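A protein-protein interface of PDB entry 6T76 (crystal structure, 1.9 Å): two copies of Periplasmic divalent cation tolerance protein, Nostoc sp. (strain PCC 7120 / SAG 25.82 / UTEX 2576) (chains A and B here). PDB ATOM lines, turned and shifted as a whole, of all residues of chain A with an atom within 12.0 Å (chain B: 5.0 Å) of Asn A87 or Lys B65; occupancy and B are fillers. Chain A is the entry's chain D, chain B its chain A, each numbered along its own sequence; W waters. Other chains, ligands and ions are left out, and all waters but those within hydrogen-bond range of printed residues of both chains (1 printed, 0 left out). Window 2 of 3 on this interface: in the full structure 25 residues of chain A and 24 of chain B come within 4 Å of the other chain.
The side-chain amino group of Lys B65 is in hydrogen-bond range of the backbone carbonyl oxygen of Ser A89.
The backbone NH (N) of Leu A90 is in hydrogen-bond range of the backbone carbonyl oxygen (O) of Phe B79 (3.0 Å).
The side-chain amino group (NZ) of Lys B65 lies within hydrogen-bond range of the backbone carbonyl oxygen (O) of Ala A88, at 3.3 Å.
OG of Ser A89 lies within hydrogen-bond range of O of Asp A85 (2.7 Å).
N of Ala A88 sits at hydrogen-bond distance from OD1 of Asp A85, at 3.0 Å.
OD1 of Asp A85 lies close to N of Asn A87, at 3.3 Å.
The side-chain carboxylate (OE1) of Glu B62 lies within salt-bridge range of the side-chain amino group (NZ) of Lys B65, at 3.97 Å.
The side-chain sulfur (SG) of Cys B69 is in hydrogen-bond range of the backbone carbonyl oxygen (O) of Lys B65.
Among the printed residues, merely in contact across the chains: Ser A89 with Phe B79 (3.4 Å), Ala A88 with Phe B79 (3.6 Å), Ala A88 with Ile B61 (3.8 Å), Asn A87 with Lys B65 (3.9 Å), Leu A90 with Lys B65 (3.9 Å) and Leu A90 with Cys B69 (3.9 Å).
Lys B65 touches just these residues of chain A: Asn A87 (3.9 Å), Ala A88 (3.3 Å), Ser A89 (3.0 Å) and Leu A90 (3.9 Å).
Ile B61 touches just one residue of chain A: Ala A88 (3.8 Å).
No residue of chain A comes within 4 Å of Glu B62.
No residue of chain A comes within 4 Å of Leu B64.
No residue of chain A comes within 4 Å of Gln B66.
No residue of chain A comes within 4 Å of Ile B68.
Phe B79 touches just these residues of chain A: Ala A88 (3.6 Å), Ser A89 (3.4 Å) and Leu A90 (3.0 Å).
Printed residues of chain B within 4 Å of Leu A90: Lys B65, Cys B69 and Phe B79.
Of the printed residues of chain B, Ser A89 touches Lys B65 (3.0 Å) and Phe B79 (3.4 Å).
Glu A83 touches none of the printed residues of chain B.
The nearest printed residue of chain B that does not touch Asn A87 is Glu B62 (5.4 Å).
Hydrophobic or aromatic side chains of chain A that line the printed part of chain B: Ala A88 and Leu A90.
Of the 10 printed residues of chain B, 4 touch a printed residue of chain A.
Hydrophobic or aromatic side chains of chain B that line the printed part of chain A: Ile B61 and Phe B79.
Along chain B the printed residues that touch a printed residue of chain A span positions 61 to 79.
No position is printed for both chains.
Water W1 lies within hydrogen-bond range of NZ of Lys B65 (2.8 Å) and N of Arg A91 (3.1 Å).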
ATOM      1  N   MET A   1      18.453  28.780   5.863  1.00  0.00           N
ATOM      2  CA  MET A   1      18.866  29.153   4.499  1.00  0.00           C
ATOM      3  C   MET A   1      17.819  28.594   3.539  1.00  0.00           C
ATOM      4  O   MET A   1      17.031  27.745   3.917  1.00  0.00           O
ATOM      5  CB  MET A   1      20.258  28.606   4.200  1.00  0.00           C
ATOM      6  CG  MET A   1      20.260  27.117   3.970  1.00  0.00           C
ATOM      7  SD  MET A   1      21.825  26.447   3.384  1.00  0.00           S
ATOM      8  CE  MET A   1      21.672  26.805   1.645  1.00  0.00           C
ATOM      9  N   LYS A   2      17.836  29.068   2.298  1.00  0.00           N
ATOM     10  CA  LYS A   2      17.058  28.474   1.238  1.00  0.00           C
ATOM     11  C   LYS A   2      17.960  28.452  -0.028  1.00  0.00           C
ATOM     12  O   LYS A   2      19.056  28.954  -0.028  1.00  0.00           O
ATOM     13  CB  LYS A   2      15.737  29.238   0.941  1.00  0.00           C
ATOM     14  CG  LYS A   2      14.600  29.094   2.041  1.00  0.00           C
ATOM     15  CD  LYS A   2      13.162  29.692   1.781  1.00  0.00           C
ATOM     16  N   THR A  58      17.666  32.737   4.738  1.00  0.00           N
ATOM     17  CA  THR A  58      16.243  32.876   4.543  1.00  0.00           C
ATOM     18  C   THR A  58      15.868  34.347   4.579  1.00  0.00           C
ATOM     19  O   THR A  58      15.071  34.835   3.755  1.00  0.00           O
ATOM     20  CB  THR A  58      15.472  32.002   5.562  1.00  0.00           C
ATOM     21  OG1 THR A  58      15.709  30.667   5.205  1.00  0.00           O
ATOM     22  CG2 THR A  58      13.969  32.289   5.560  1.00  0.00           C
ATOM     23  N   ILE A  82      13.494  26.990  -3.440  1.00  0.00           N
ATOM     24  CA  ILE A  82      13.345  25.624  -3.022  1.00  0.00           C
ATOM     25  C   ILE A  82      13.558  25.555  -1.533  1.00  0.00           C
ATOM     26  O   ILE A  82      14.510  26.137  -0.992  1.00  0.00           O
ATOM     27  CB  ILE A  82      14.431  24.800  -3.729  1.00  0.00           C
ATOM     28  CG1 ILE A  82      14.216  24.761  -5.235  1.00  0.00           C
ATOM     29  CG2 ILE A  82      14.510  23.368  -3.158  1.00  0.00           C
ATOM     30  CD1 ILE A  82      15.365  23.979  -5.921  1.00  0.00           C
ATOM     31  N   GLU A  83      12.703  24.826  -0.852  1.00  0.00           N
ATOM     32  CA  GLU A  83      12.758  24.674   0.595  1.00  0.00           C
ATOM     33  C   GLU A  83      13.860  23.756   1.028  1.00  0.00           C
ATOM     34  O   GLU A  83      13.951  22.650   0.555  1.00  0.00           O
ATOM     35  CB  GLU A  83      11.407  24.088   1.085  1.00  0.00           C
ATOM     36  CG  GLU A  83      10.378  25.100   0.704  1.00  0.00           C
ATOM     37  CD  GLU A  83       9.084  24.964   1.422  1.00  0.00           C
ATOM     38  OE1 GLU A  83       8.886  23.879   1.972  1.00  0.00           O
ATOM     39  OE2 GLU A  83       8.311  25.960   1.411  1.00  0.00           O
ATOM     40  N   VAL A  84      14.638  24.221   1.989  1.00  0.00           N
ATOM     41  CA  VAL A  84      15.700  23.473   2.653  1.00  0.00           C
ATOM     42  C   VAL A  84      15.275  22.965   4.008  1.00  0.00           C
ATOM     43  O   VAL A  84      14.621  23.665   4.743  1.00  0.00           O
ATOM     44  CB  VAL A  84      16.931  24.377   2.768  1.00  0.00           C
ATOM     45  CG1 VAL A  84      17.996  23.768   3.649  1.00  0.00           C
ATOM     46  CG2 VAL A  84      17.467  24.644   1.385  1.00  0.00           C
ATOM     47  N   ASP A  85      15.612  21.719   4.314  1.00  0.00           N
ATOM     48  CA  ASP A  85      15.434  21.179   5.632  1.00  0.00           C
ATOM     49  C   ASP A  85      16.623  21.668   6.461  1.00  0.00           C
ATOM     50  O   ASP A  85      17.684  21.018   6.466  1.00  0.00           O
ATOM     51  CB  ASP A  85      15.323  19.656   5.600  1.00  0.00           C
ATOM     52  CG  ASP A  85      15.018  19.047   6.953  1.00  0.00           C
ATOM     53  OD1 ASP A  85      15.265  19.634   8.024  1.00  0.00           O
ATOM     54  OD2 ASP A  85      14.607  17.892   6.978  1.00  0.00           O
ATOM     55  N   ASN A  86      16.414  22.796   7.161  1.00  0.00           N
ATOM     56  CA  ASN A  86      17.478  23.420   7.956  1.00  0.00           C
ATOM     57  C   ASN A  86      17.995  22.578   9.133  1.00  0.00           C
ATOM     58  O   ASN A  86      19.192  22.533   9.412  1.00  0.00           O
ATOM     59  CB  ASN A  86      17.119  24.867   8.352  1.00  0.00           C
ATOM     60  CG  ASN A  86      17.305  25.844   7.175  1.00  0.00           C
ATOM     61  OD1 ASN A  86      18.410  26.207   6.843  1.00  0.00           O
ATOM     62  ND2 ASN A  86      16.246  26.175   6.493  1.00  0.00           N
ATOM     63  N   ASN A  87      17.123  21.801   9.739  1.00  0.00           N
ATOM     64  CA  ASN A  87      17.530  20.902  10.814  1.00  0.00           C
ATOM     65  C   ASN A  87      18.351  19.728  10.362  1.00  0.00           C
ATOM     66  O   ASN A  87      19.261  19.326  11.044  1.00  0.00           O
ATOM     67  CB  ASN A  87      16.289  20.459  11.575  1.00  0.00           C
ATOM     68  CG  ASN A  87      15.741  21.583  12.415  1.00  0.00           C
ATOM     69  OD1 ASN A  87      16.340  22.681  12.544  1.00  0.00           O
ATOM     70  ND2 ASN A  87      14.587  21.357  12.957  1.00  0.00           N
ATOM     71  N   ALA A  88      18.027  19.159   9.221  1.00  0.00           N
ATOM     72  CA  ALA A  88      18.750  18.007   8.769  1.00  0.00           C
ATOM     73  C   ALA A  88      20.106  18.419   8.119  1.00  0.00           C
ATOM     74  O   ALA A  88      21.007  17.581   8.008  1.00  0.00           O
ATOM     75  CB  ALA A  88      17.898  17.211   7.773  1.00  0.00           C
ATOM     76  N   SER A  89      20.193  19.652   7.632  1.00  0.00           N
ATOM     77  CA  SER A  89      21.401  20.165   7.002  1.00  0.00           C
ATOM     78  C   SER A  89      22.478  20.365   8.053  1.00  0.00           C
ATOM     79  O   SER A  89      22.189  20.319   9.256  1.00  0.00           O
ATOM     80  CB  SER A  89      21.137  21.466   6.278  1.00  0.00           C
ATOM     81  OG  SER A  89      20.138  21.376   5.319  1.00  0.00           O
ATOM     82  N   LEU A  90      23.720  20.587   7.609  1.00  0.00           N
ATOM     83  CA  LEU A  90      24.831  20.751   8.526  1.00  0.00           C
ATOM     84  C   LEU A  90      24.743  22.183   9.067  1.00  0.00           C
ATOM     85  O   LEU A  90      24.745  23.159   8.300  1.00  0.00           O
ATOM     86  CB  LEU A  90      26.176  20.513   7.840  1.00  0.00           C
ATOM     87  CG  LEU A  90      27.399  20.593   8.748  1.00  0.00           C
ATOM     88  CD1 LEU A  90      27.451  19.478   9.759  1.00  0.00           C
ATOM     89  CD2 LEU A  90      28.654  20.564   7.867  1.00  0.00           C
ATOM     90  N   ARG A  91      24.607  22.278  10.364  1.00  0.00           N
ATOM     91  CA  ARG A  91      24.358  23.567  11.038  1.00  0.00           C
ATOM     92  C   ARG A  91      25.462  24.606  10.806  1.00  0.00           C
ATOM     93  O   ARG A  91      25.169  25.738  10.487  1.00  0.00           O
ATOM     94  CB  ARG A  91      24.203  23.296  12.529  1.00  0.00           C
ATOM     95  CG  ARG A  91      24.180  24.547  13.350  1.00  0.00           C
ATOM     96  CD  ARG A  91      22.747  25.068  13.245  1.00  0.00           C
ATOM     97  NE  ARG A  91      22.152  24.534  14.501  1.00  0.00           N
ATOM     98  CZ  ARG A  91      21.157  23.643  14.679  1.00  0.00           C
ATOM     99  NH1 ARG A  91      20.465  23.115  13.658  1.00  0.00           N
ATOM    100  NH2 ARG A  91      20.806  23.326  15.946  1.00  0.00           N
ATOM    101  N   GLU A  92      26.736  24.181  10.901  1.00  0.00           N
ATOM    102  CA  GLU A  92      27.900  25.053  10.580  1.00  0.00           C
ATOM    103  C   GLU A  92      27.807  25.599   9.140  1.00  0.00           C
ATOM    104  O   GLU A  92      28.117  26.769   8.883  1.00  0.00           O
ATOM    105  CB  GLU A  92      29.254  24.364  10.873  1.00  0.00           C
ATOM    106  CG  GLU A  92      29.703  23.219   9.953  1.00  0.00           C
ATOM    107  CD  GLU A  92      31.008  22.565  10.462  1.00  0.00           C
ATOM    108  OE1 GLU A  92      31.866  22.047   9.686  1.00  0.00           O
ATOM    109  OE2 GLU A  92      31.177  22.569  11.696  1.00  0.00           O
ATOM    110  N   TYR A  93      27.295  24.805   8.204  1.00  0.00           N
ATOM    111  CA  TYR A  93      27.138  25.299   6.839  1.00  0.00           C
ATOM    112  C   TYR A  93      26.027  26.372   6.715  1.00  0.00           C
ATOM    113  O   TYR A  93      26.202  27.392   6.052  1.00  0.00           O
ATOM    114  CB  TYR A  93      26.918  24.172   5.824  1.00  0.00           C
ATOM    115  CG  TYR A  93      26.939  24.728   4.433  1.00  0.00           C
ATOM    116  CD1 TYR A  93      28.163  25.075   3.817  1.00  0.00           C
ATOM    117  CD2 TYR A  93      25.769  24.924   3.721  1.00  0.00           C
ATOM    118  CE1 TYR A  93      28.174  25.600   2.534  1.00  0.00           C
ATOM    119  CE2 TYR A  93      25.775  25.467   2.433  1.00  0.00           C
ATOM    120  CZ  TYR A  93      26.974  25.798   1.841  1.00  0.00           C
ATOM    121  OH  TYR A  93      26.960  26.321   0.568  1.00  0.00           O
ATOM    122  N   ILE A  94      24.907  26.121   7.361  1.00  0.00           N
ATOM    123  CA  ILE A  94      23.793  27.072   7.341  1.00  0.00           C
ATOM    124  C   ILE A  94      24.171  28.371   8.026  1.00  0.00           C
ATOM    125  O   ILE A  94      23.851  29.427   7.541  1.00  0.00           O
ATOM    126  CB  ILE A  94      22.598  26.477   8.128  1.00  0.00           C
ATOM    127  CG1 ILE A  94      21.946  25.376   7.320  1.00  0.00           C
ATOM    128  CG2 ILE A  94      21.610  27.553   8.554  1.00  0.00           C
ATOM    129  CD1 ILE A  94      20.936  24.679   8.193  1.00  0.00           C
ATOM    130  N   ASP A  95      24.935  28.284   9.101  1.00  0.00           N
ATOM    131  CA  ASP A  95      25.521  29.466   9.711  1.00  0.00           C
ATOM    132  C   ASP A  95      26.518  30.224   8.791  1.00  0.00           C
ATOM    133  O   ASP A  95      26.553  31.430   8.794  1.00  0.00           O
ATOM    134  CB  ASP A  95      26.207  29.086  11.032  1.00  0.00           C
ATOM    135  CG  ASP A  95      25.213  28.650  12.109  1.00  0.00           C
ATOM    136  OD1 ASP A  95      24.002  28.892  11.970  1.00  0.00           O
ATOM    137  OD2 ASP A  95      25.662  28.055  13.102  1.00  0.00           O
ATOM    138  N   ILE B  61      19.291  10.126   6.901  1.00  0.00           N
ATOM    139  CA  ILE B  61      19.939  11.443   6.691  1.00  0.00           C
ATOM    140  C   ILE B  61      21.078  11.731   7.682  1.00  0.00           C
ATOM    141  O   ILE B  61      22.103  12.244   7.307  1.00  0.00           O
ATOM    142  CB  ILE B  61      18.953  12.641   6.805  1.00  0.00           C
ATOM    143  CG1 ILE B  61      18.226  12.848   5.522  1.00  0.00           C
ATOM    144  CG2 ILE B  61      19.701  13.964   7.006  1.00  0.00           C
ATOM    145  CD1 ILE B  61      19.137  13.404   4.412  1.00  0.00           C
ATOM    146  N   GLU B  62      20.880  11.417   8.945  1.00  0.00           N
ATOM    147  CA  GLU B  62      21.880  11.661   9.936  1.00  0.00           C
ATOM    148  C   GLU B  62      23.156  10.853   9.680  1.00  0.00           C
ATOM    149  O   GLU B  62      24.265  11.363   9.845  1.00  0.00           O
ATOM    150  CB  GLU B  62      21.321  11.354  11.318  1.00  0.00           C
ATOM    151  CG  GLU B  62      22.058  12.098  12.380  1.00  0.00           C
ATOM    152  CD  GLU B  62      22.110  13.590  12.123  1.00  0.00           C
ATOM    153  OE1 GLU B  62      23.260  14.058  12.109  1.00  0.00           O
ATOM    154  OE2 GLU B  62      21.070  14.264  11.909  1.00  0.00           O
ATOM    155  N   ARG B  63      23.005   9.576   9.359  1.00  0.00           N
ATOM    156  CA  ARG B  63      24.145   8.739   9.059  1.00  0.00           C
ATOM    157  C   ARG B  63      24.893   9.276   7.829  1.00  0.00           C
ATOM    158  O   ARG B  63      26.132   9.272   7.794  1.00  0.00           O
ATOM    159  CB  ARG B  63      23.698   7.294   8.858  1.00  0.00           C
ATOM    160  CG  ARG B  63      24.816   6.335   8.467  1.00  0.00           C
ATOM    161  CD  ARG B  63      24.317   4.882   8.435  1.00  0.00           C
ATOM    162  NE  ARG B  63      25.217   3.884   7.856  1.00  0.00           N
ATOM    163  CZ  ARG B  63      24.838   2.693   7.346  1.00  0.00           C
ATOM    164  N   LEU B  64      24.151   9.744   6.830  1.00  0.00           N
ATOM    165  CA  LEU B  64      24.788  10.363   5.677  1.00  0.00           C
ATOM    166  C   LEU B  64      25.567  11.568   6.058  1.00  0.00           C
ATOM    167  O   LEU B  64      26.723  11.773   5.598  1.00  0.00           O
ATOM    168  CB  LEU B  64      23.778  10.737   4.615  1.00  0.00           C
ATOM    169  CG  LEU B  64      24.259  11.521   3.417  1.00  0.00           C
ATOM    170  CD1 LEU B  64      25.353  10.752   2.676  1.00  0.00           C
ATOM    171  CD2 LEU B  64      23.120  11.843   2.475  1.00  0.00           C
ATOM    172  N   LYS B  65      24.964  12.424   6.876  1.00  0.00           N
ATOM    173  CA  LYS B  65      25.619  13.649   7.272  1.00  0.00           C
ATOM    174  C   LYS B  65      26.948  13.320   7.946  1.00  0.00           C
ATOM    175  O   LYS B  65      27.953  14.000   7.714  1.00  0.00           O
ATOM    176  CB  LYS B  65      24.716  14.516   8.169  1.00  0.00           C
ATOM    177  CG  LYS B  65      25.413  15.762   8.743  1.00  0.00           C
ATOM    178  CD  LYS B  65      24.438  16.899   9.133  1.00  0.00           C
ATOM    179  CE  LYS B  65      23.640  16.590  10.354  1.00  0.00           C
ATOM    180  NZ  LYS B  65      22.800  17.751  10.723  1.00  0.00           N
ATOM    181  N   GLN B  66      26.923  12.357   8.835  1.00  0.00           N
ATOM    182  CA  GLN B  66      28.102  11.997   9.604  1.00  0.00           C
ATOM    183  C   GLN B  66      29.204  11.490   8.641  1.00  0.00           C
ATOM    184  O   GLN B  66      30.374  11.853   8.763  1.00  0.00           O
ATOM    185  CB  GLN B  66      27.760  10.875  10.588  1.00  0.00           C
ATOM    186  CG  GLN B  66      26.896  11.193  11.813  1.00  0.00           C
ATOM    187  CD  GLN B  66      27.070  12.589  12.363  1.00  0.00           C
ATOM    188  OE1 GLN B  66      26.171  13.466  12.277  1.00  0.00           O
ATOM    189  NE2 GLN B  66      28.217  12.799  12.953  1.00  0.00           N
ATOM    190  N   ARG B  67      28.811  10.619   7.731  1.00  0.00           N
ATOM    191  CA  ARG B  67      29.788  10.037   6.785  1.00  0.00           C
ATOM    192  C   ARG B  67      30.382  11.053   5.819  1.00  0.00           C
ATOM    193  O   ARG B  67      31.598  11.077   5.594  1.00  0.00           O
ATOM    194  CB  ARG B  67      29.150   8.930   5.988  1.00  0.00           C
ATOM    195  CG  ARG B  67      30.194   8.071   5.255  1.00  0.00           C
ATOM    196  CD  ARG B  67      30.837   7.066   6.186  1.00  0.00           C
ATOM    197  NE  ARG B  67      31.771   6.309   5.362  1.00  0.00           N
ATOM    198  CZ  ARG B  67      33.102   6.361   5.443  1.00  0.00           C
ATOM    199  NH1 ARG B  67      33.723   7.113   6.384  1.00  0.00           N
ATOM    200  NH2 ARG B  67      33.832   5.616   4.609  1.00  0.00           N
ATOM    201  N   ILE B  68      29.545  11.942   5.288  1.00  0.00           N
ATOM    202  CA  ILE B  68      30.043  13.136   4.573  1.00  0.00           C
ATOM    203  C   ILE B  68      31.068  13.924   5.365  1.00  0.00           C
ATOM    204  O   ILE B  68      32.122  14.288   4.841  1.00  0.00           O
ATOM    205  CB  ILE B  68      28.885  14.100   4.148  1.00  0.00           C
ATOM    206  CG1 ILE B  68      28.054  13.457   3.069  1.00  0.00           C
ATOM    207  CG2 ILE B  68      29.428  15.456   3.637  1.00  0.00           C
ATOM    208  CD1 ILE B  68      28.816  13.239   1.770  1.00  0.00           C
ATOM    209  N   CYS B  69      30.785  14.250   6.611  1.00  0.00           N
ATOM    210  CA  CYS B  69      31.744  15.016   7.397  1.00  0.00           C
ATOM    211  C   CYS B  69      33.003  14.227   7.637  1.00  0.00           C
ATOM    212  O   CYS B  69      34.057  14.826   7.799  1.00  0.00           O
ATOM    213  CB  CYS B  69      31.128  15.454   8.734  1.00  0.00           C
ATOM    214  SG  CYS B  69      29.802  16.652   8.351  1.00  0.00           S
ATOM    215  N   PHE B  79      26.597  20.682   3.234  1.00  0.00           N
ATOM    216  CA  PHE B  79      25.645  19.586   3.330  1.00  0.00           C
ATOM    217  C   PHE B  79      24.280  20.186   3.523  1.00  0.00           C
ATOM    218  O   PHE B  79      23.954  20.688   4.608  1.00  0.00           O
ATOM    219  CB  PHE B  79      26.006  18.642   4.443  1.00  0.00           C
ATOM    220  CG  PHE B  79      25.129  17.470   4.495  1.00  0.00           C
ATOM    221  CD1 PHE B  79      25.317  16.405   3.627  1.00  0.00           C
ATOM    222  CD2 PHE B  79      24.069  17.415   5.376  1.00  0.00           C
ATOM    223  CE1 PHE B  79      24.457  15.290   3.678  1.00  0.00           C
ATOM    224  CE2 PHE B  79      23.247  16.302   5.445  1.00  0.00           C
ATOM    225  CZ  PHE B  79      23.428  15.257   4.595  1.00  0.00           C
HETATM  226  O   HOH W   1      24.351  19.693  12.044  1.00  0.00           O
